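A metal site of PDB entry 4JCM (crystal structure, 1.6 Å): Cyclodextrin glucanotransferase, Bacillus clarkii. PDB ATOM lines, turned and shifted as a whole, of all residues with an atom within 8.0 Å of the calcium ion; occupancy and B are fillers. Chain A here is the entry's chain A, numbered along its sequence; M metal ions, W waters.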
ATOM      1  N   PRO A 163     -37.093  20.336 -10.590  1.00  0.00           N
ATOM      2  CA  PRO A 163     -36.879  21.504 -11.468  1.00  0.00           C
ATOM      3  C   PRO A 163     -35.409  21.746 -11.817  1.00  0.00           C
ATOM      4  O   PRO A 163     -35.100  22.718 -12.543  1.00  0.00           O
ATOM      5  CB  PRO A 163     -37.429  22.676 -10.644  1.00  0.00           C
ATOM      6  CG  PRO A 163     -37.338  22.234  -9.231  1.00  0.00           C
ATOM      7  CD  PRO A 163     -37.429  20.720  -9.209  1.00  0.00           C
ATOM      8  N   ASN A 164     -34.529  20.887 -11.330  1.00  0.00           N
ATOM      9  CA  ASN A 164     -33.095  21.072 -11.531  1.00  0.00           C
ATOM     10  C   ASN A 164     -32.570  20.647 -12.906  1.00  0.00           C
ATOM     11  O   ASN A 164     -31.611  21.225 -13.419  1.00  0.00           O
ATOM     12  CB  ASN A 164     -32.296  20.334 -10.472  1.00  0.00           C
ATOM     13  CG  ASN A 164     -30.818  20.661 -10.537  1.00  0.00           C
ATOM     14  OD1 ASN A 164     -30.435  21.819 -10.340  1.00  0.00           O
ATOM     15  ND2 ASN A 164     -29.998  19.669 -10.827  1.00  0.00           N
ATOM     16  N   HIS A 165     -33.171  19.623 -13.471  1.00  0.00           N
ATOM     17  CA  HIS A 165     -32.591  19.006 -14.648  1.00  0.00           C
ATOM     18  C   HIS A 165     -33.615  18.224 -15.443  1.00  0.00           C
ATOM     19  O   HIS A 165     -34.702  17.908 -14.951  1.00  0.00           O
ATOM     20  CB  HIS A 165     -31.441  18.066 -14.254  1.00  0.00           C
ATOM     21  CG  HIS A 165     -31.802  17.053 -13.204  1.00  0.00           C
ATOM     22  ND1 HIS A 165     -32.442  15.875 -13.505  1.00  0.00           N
ATOM     23  CD2 HIS A 165     -31.617  17.053 -11.867  1.00  0.00           C
ATOM     24  CE1 HIS A 165     -32.627  15.182 -12.389  1.00  0.00           C
ATOM     25  NE2 HIS A 165     -32.127  15.882 -11.381  1.00  0.00           N
ATOM     26  N   TYR A 195     -27.906  25.264 -18.304  1.00  0.00           N
ATOM     27  CA  TYR A 195     -26.560  25.647 -17.878  1.00  0.00           C
ATOM     28  C   TYR A 195     -25.546  24.686 -18.486  1.00  0.00           C
ATOM     29  O   TYR A 195     -25.646  23.473 -18.304  1.00  0.00           O
ATOM     30  CB  TYR A 195     -26.428  25.583 -16.361  1.00  0.00           C
ATOM     31  CG  TYR A 195     -27.088  26.724 -15.610  1.00  0.00           C
ATOM     32  CD1 TYR A 195     -26.721  28.046 -15.844  1.00  0.00           C
ATOM     33  CD2 TYR A 195     -28.046  26.472 -14.639  1.00  0.00           C
ATOM     34  CE1 TYR A 195     -27.306  29.089 -15.149  1.00  0.00           C
ATOM     35  CE2 TYR A 195     -28.642  27.505 -13.942  1.00  0.00           C
ATOM     36  CZ  TYR A 195     -28.270  28.817 -14.203  1.00  0.00           C
ATOM     37  OH  TYR A 195     -28.855  29.846 -13.513  1.00  0.00           O
ATOM     38  N   GLU A 206     -21.068  26.832  -4.912  1.00  0.00           N
ATOM     39  CA  GLU A 206     -21.283  27.472  -6.199  1.00  0.00           C
ATOM     40  C   GLU A 206     -21.236  26.458  -7.341  1.00  0.00           C
ATOM     41  O   GLU A 206     -22.107  26.431  -8.221  1.00  0.00           O
ATOM     42  CB  GLU A 206     -20.239  28.580  -6.420  1.00  0.00           C
ATOM     43  CG  GLU A 206     -20.444  29.376  -7.691  1.00  0.00           C
ATOM     44  CD  GLU A 206     -19.412  30.483  -7.860  1.00  0.00           C
ATOM     45  OE1 GLU A 206     -18.629  30.734  -6.913  1.00  0.00           O
ATOM     46  OE2 GLU A 206     -19.395  31.098  -8.941  1.00  0.00           O
ATOM     47  N   ASN A 207     -20.206  25.623  -7.352  1.00  0.00           N
ATOM     48  CA  ASN A 207     -20.082  24.606  -8.381  1.00  0.00           C
ATOM     49  C   ASN A 207     -21.202  23.580  -8.294  1.00  0.00           C
ATOM     50  O   ASN A 207     -21.635  23.039  -9.312  1.00  0.00           O
ATOM     51  CB  ASN A 207     -18.703  23.946  -8.323  1.00  0.00           C
ATOM     52  CG  ASN A 207     -17.640  24.787  -8.980  1.00  0.00           C
ATOM     53  OD1 ASN A 207     -17.274  25.852  -8.496  1.00  0.00           O
ATOM     54  ND2 ASN A 207     -17.120  24.317 -10.107  1.00  0.00           N
ATOM     55  N   SER A 208     -21.688  23.342  -7.079  1.00  0.00           N
ATOM     56  CA  SER A 208     -22.742  22.357  -6.855  1.00  0.00           C
ATOM     57  C   SER A 208     -24.059  22.841  -7.465  1.00  0.00           C
ATOM     58  O   SER A 208     -24.924  22.042  -7.809  1.00  0.00           O
ATOM     59  CB  SER A 208     -22.938  22.123  -5.360  1.00  0.00           C
ATOM     60  OG  SER A 208     -21.797  21.497  -4.800  1.00  0.00           O
ATOM     61  N   ILE A 209     -24.172  24.154  -7.617  1.00  0.00           N
ATOM     62  CA  ILE A 209     -25.392  24.760  -8.150  1.00  0.00           C
ATOM     63  C   ILE A 209     -25.361  24.926  -9.669  1.00  0.00           C
ATOM     64  O   ILE A 209     -26.328  24.607 -10.359  1.00  0.00           O
ATOM     65  CB  ILE A 209     -25.683  26.126  -7.501  1.00  0.00           C
ATOM     66  CG1 ILE A 209     -26.037  25.922  -6.025  1.00  0.00           C
ATOM     67  CG2 ILE A 209     -26.811  26.835  -8.235  1.00  0.00           C
ATOM     68  CD1 ILE A 209     -26.004  27.204  -5.196  1.00  0.00           C
ATOM     69  N   TYR A 210     -24.251  25.428 -10.200  1.00  0.00           N
ATOM     70  CA  TYR A 210     -24.234  25.823 -11.607  1.00  0.00           C
ATOM     71  C   TYR A 210     -23.600  24.812 -12.569  1.00  0.00           C
ATOM     72  O   TYR A 210     -23.808  24.886 -13.776  1.00  0.00           O
ATOM     73  CB  TYR A 210     -23.622  27.208 -11.768  1.00  0.00           C
ATOM     74  CG  TYR A 210     -24.439  28.275 -11.080  1.00  0.00           C
ATOM     75  CD1 TYR A 210     -25.612  28.754 -11.641  1.00  0.00           C
ATOM     76  CD2 TYR A 210     -24.045  28.788  -9.840  1.00  0.00           C
ATOM     77  CE1 TYR A 210     -26.367  29.717 -10.998  1.00  0.00           C
ATOM     78  CE2 TYR A 210     -24.788  29.760  -9.199  1.00  0.00           C
ATOM     79  CZ  TYR A 210     -25.959  30.219  -9.783  1.00  0.00           C
ATOM     80  OH  TYR A 210     -26.711  31.179  -9.150  1.00  0.00           O
ATOM     81  N   ARG A 211     -22.841  23.861 -12.033  1.00  0.00           N
ATOM     82  CA  ARG A 211     -22.316  22.772 -12.852  1.00  0.00           C
ATOM     83  C   ARG A 211     -23.252  21.561 -12.743  1.00  0.00           C
ATOM     84  O   ARG A 211     -24.070  21.493 -11.823  1.00  0.00           O
ATOM     85  CB  ARG A 211     -20.886  22.425 -12.431  1.00  0.00           C
ATOM     86  CG  ARG A 211     -20.037  23.669 -12.119  1.00  0.00           C
ATOM     87  CD  ARG A 211     -18.590  23.533 -12.559  1.00  0.00           C
ATOM     88  NE  ARG A 211     -18.274  24.404 -13.691  1.00  0.00           N
ATOM     89  CZ  ARG A 211     -17.395  25.391 -13.673  1.00  0.00           C
ATOM     90  NH1 ARG A 211     -17.194  26.129 -14.750  1.00  0.00           N
ATOM     91  NH2 ARG A 211     -16.707  25.656 -12.563  1.00  0.00           N
ATOM     92  N   ASN A 212     -23.160  20.627 -13.681  1.00  0.00           N
ATOM     93  CA  ASN A 212     -24.115  19.509 -13.735  1.00  0.00           C
ATOM     94  C   ASN A 212     -24.059  18.555 -12.547  1.00  0.00           C
ATOM     95  O   ASN A 212     -22.994  18.236 -12.039  1.00  0.00           O
ATOM     96  CB  ASN A 212     -23.947  18.699 -15.028  1.00  0.00           C
ATOM     97  CG  ASN A 212     -24.380  19.465 -16.251  1.00  0.00           C
ATOM     98  OD1 ASN A 212     -25.200  20.384 -16.183  1.00  0.00           O
ATOM     99  ND2 ASN A 212     -23.827  19.089 -17.400  1.00  0.00           N
ATOM    100  N   LEU A 213     -25.245  18.125 -12.113  1.00  0.00           N
ATOM    101  CA  LEU A 213     -25.368  17.037 -11.154  1.00  0.00           C
ATOM    102  C   LEU A 213     -25.126  15.741 -11.927  1.00  0.00           C
ATOM    103  O   LEU A 213     -25.913  15.375 -12.806  1.00  0.00           O
ATOM    104  CB  LEU A 213     -26.770  17.059 -10.538  1.00  0.00           C
ATOM    105  CG  LEU A 213     -27.119  16.119  -9.373  1.00  0.00           C
ATOM    106  CD1 LEU A 213     -26.193  16.361  -8.189  1.00  0.00           C
ATOM    107  CD2 LEU A 213     -28.583  16.318  -8.973  1.00  0.00           C
ATOM    108  N   ALA A 217     -28.599  16.985 -17.551  1.00  0.00           N
ATOM    109  CA  ALA A 217     -28.697  18.288 -18.211  1.00  0.00           C
ATOM    110  C   ALA A 217     -29.335  19.310 -17.276  1.00  0.00           C
ATOM    111  O   ALA A 217     -30.535  19.263 -17.012  1.00  0.00           O
ATOM    112  CB  ALA A 217     -29.531  18.166 -19.493  1.00  0.00           C
ATOM    113  N   SER A 218     -28.534  20.264 -16.810  1.00  0.00           N
ATOM    114  CA  SER A 218     -29.007  21.281 -15.876  1.00  0.00           C
ATOM    115  C   SER A 218     -29.895  22.333 -16.542  1.00  0.00           C
ATOM    116  O   SER A 218     -29.460  22.991 -17.500  1.00  0.00           O
ATOM    117  CB  SER A 218     -27.822  22.012 -15.228  1.00  0.00           C
ATOM    118  OG  SER A 218     -27.092  21.142 -14.380  1.00  0.00           O
ATOM    119  N   LEU A 219     -31.117  22.497 -16.041  1.00  0.00           N
ATOM    120  CA  LEU A 219     -31.991  23.562 -16.524  1.00  0.00           C
ATOM    121  C   LEU A 219     -31.504  24.919 -16.016  1.00  0.00           C
ATOM    122  O   LEU A 219     -31.050  25.038 -14.877  1.00  0.00           O
ATOM    123  CB  LEU A 219     -33.439  23.342 -16.080  1.00  0.00           C
ATOM    124  CG  LEU A 219     -34.157  22.211 -16.809  1.00  0.00           C
ATOM    125  CD1 LEU A 219     -35.460  21.829 -16.099  1.00  0.00           C
ATOM    126  CD2 LEU A 219     -34.419  22.600 -18.264  1.00  0.00           C
ATOM    127  N   ASN A 220     -31.594  25.929 -16.873  1.00  0.00           N
ATOM    128  CA  ASN A 220     -31.271  27.287 -16.461  1.00  0.00           C
ATOM    129  C   ASN A 220     -32.525  27.944 -15.903  1.00  0.00           C
ATOM    130  O   ASN A 220     -33.264  28.568 -16.664  1.00  0.00           O
ATOM    131  CB  ASN A 220     -30.734  28.065 -17.657  1.00  0.00           C
ATOM    132  CG  ASN A 220     -30.377  29.522 -17.313  1.00  0.00           C
ATOM    133  OD1 ASN A 220     -30.408  29.926 -16.147  1.00  0.00           O
ATOM    134  ND2 ASN A 220     -30.031  30.300 -18.335  1.00  0.00           N
ATOM    135  N   GLN A 221     -32.755  27.820 -14.591  1.00  0.00           N
ATOM    136  CA  GLN A 221     -34.000  28.315 -13.998  1.00  0.00           C
ATOM    137  C   GLN A 221     -34.097  29.826 -14.053  1.00  0.00           C
ATOM    138  O   GLN A 221     -35.197  30.374 -13.971  1.00  0.00           O
ATOM    139  CB  GLN A 221     -34.155  27.866 -12.539  1.00  0.00           C
ATOM    140  CG  GLN A 221     -34.179  26.364 -12.345  1.00  0.00           C
ATOM    141  CD  GLN A 221     -32.782  25.818 -12.090  1.00  0.00           C
ATOM    142  OE1 GLN A 221     -31.815  26.571 -11.994  1.00  0.00           O
ATOM    143  NE2 GLN A 221     -32.689  24.501 -11.984  1.00  0.00           N
ATOM    144  N   ALA A 249     -33.273  17.833  -5.310  1.00  0.00           N
ATOM    145  CA  ALA A 249     -32.016  18.501  -5.598  1.00  0.00           C
ATOM    146  C   ALA A 249     -31.940  19.947  -5.146  1.00  0.00           C
ATOM    147  O   ALA A 249     -31.335  20.792  -5.821  1.00  0.00           O
ATOM    148  CB  ALA A 249     -31.702  18.408  -7.103  1.00  0.00           C
ATOM    149  N   ALA A 251     -30.246  21.156  -2.905  1.00  0.00           N
ATOM    150  CA  ALA A 251     -28.871  21.539  -2.606  1.00  0.00           C
ATOM    151  C   ALA A 251     -28.134  22.017  -3.852  1.00  0.00           C
ATOM    152  O   ALA A 251     -26.988  22.457  -3.760  1.00  0.00           O
ATOM    153  CB  ALA A 251     -28.111  20.381  -1.963  1.00  0.00           C
ATOM    154  N   HIS A 252     -28.794  21.958  -5.009  1.00  0.00           N
ATOM    155  CA  HIS A 252     -28.139  22.218  -6.290  1.00  0.00           C
ATOM    156  C   HIS A 252     -28.795  23.315  -7.108  1.00  0.00           C
ATOM    157  O   HIS A 252     -28.540  23.439  -8.296  1.00  0.00           O
ATOM    158  CB  HIS A 252     -28.069  20.929  -7.119  1.00  0.00           C
ATOM    159  CG  HIS A 252     -27.394  19.814  -6.399  1.00  0.00           C
ATOM    160  ND1 HIS A 252     -26.042  19.790  -6.158  1.00  0.00           N
ATOM    161  CD2 HIS A 252     -27.899  18.688  -5.822  1.00  0.00           C
ATOM    162  CE1 HIS A 252     -25.735  18.698  -5.480  1.00  0.00           C
ATOM    163  NE2 HIS A 252     -26.846  18.013  -5.258  1.00  0.00           N
ATOM    164  N   MET A 253     -29.654  24.110  -6.471  1.00  0.00           N
ATOM    165  CA  MET A 253     -30.286  25.254  -7.096  1.00  0.00           C
ATOM    166  C   MET A 253     -30.127  26.457  -6.168  1.00  0.00           C
ATOM    167  O   MET A 253     -30.033  26.298  -4.947  1.00  0.00           O
ATOM    168  CB  MET A 253     -31.775  24.972  -7.347  1.00  0.00           C
ATOM    169  CG  MET A 253     -32.033  23.825  -8.315  1.00  0.00           C
ATOM    170  SD  MET A 253     -33.790  23.455  -8.545  1.00  0.00           S
ATOM    171  CE  MET A 253     -34.174  22.641  -6.978  1.00  0.00           C
ATOM    172  N   PRO A 254     -30.098  27.662  -6.743  1.00  0.00           N
ATOM    173  CA  PRO A 254     -29.924  28.844  -5.892  1.00  0.00           C
ATOM    174  C   PRO A 254     -31.102  28.989  -4.937  1.00  0.00           C
ATOM    175  O   PRO A 254     -32.245  28.872  -5.346  1.00  0.00           O
ATOM    176  CB  PRO A 254     -29.910  30.010  -6.892  1.00  0.00           C
ATOM    177  CG  PRO A 254     -29.557  29.375  -8.212  1.00  0.00           C
ATOM    178  CD  PRO A 254     -30.183  28.011  -8.172  1.00  0.00           C
HETATM  179 CA    CA M   1     -28.591  23.386 -10.715  1.00  0.00          CA
HETATM  180  O   HOH W   1     -27.336  21.457 -11.486  1.00  0.00           O
HETATM  181  O   HOH W   2     -29.922  23.559 -12.865  1.00  0.00           O
HETATM  182  O   HOH W   3     -29.357  25.774 -10.657  1.00  0.00           O
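The calcium ion is bound by O of His 252 (2.4 Å), water W1 (2.4 Å), OD1 of Asn 164 (2.4 Å), water W3 (2.5 Å), water W2 (2.5 Å) and O of Ile 209 (2.6 Å). The calcium ion has six donor atoms within binding distance.
Water W2 lies within hydrogen-bond range of the backbone carbonyl oxygen (O) of Leu 219 (2.7 Å), the backbone carbonyl oxygen (O) of Asn 164 (2.9 Å) and the side-chain amide nitrogen (NE2) of Gln 221 (3.1 Å). Water W1 lies within hydrogen-bond range of OG of Ser 218 (2.9 Å), ND2 of Asn 164 (3.3 Å) and O of Arg 211 (3.3 Å).
Of the 22 residues printed, 3 come within 4 Å of the calcium ion. The nearest printed residue that does not touch the calcium ion is Met 253 (4.2 Å).
The backbone carbonyl oxygen of Ser 208 is in hydrogen-bond range of a ring nitrogen (ND1) of His 252, at 3.0 Å. The backbone carbonyl oxygen (O) of Asn 164 is in hydrogen-bond range of the backbone NH (N) of Leu 219.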
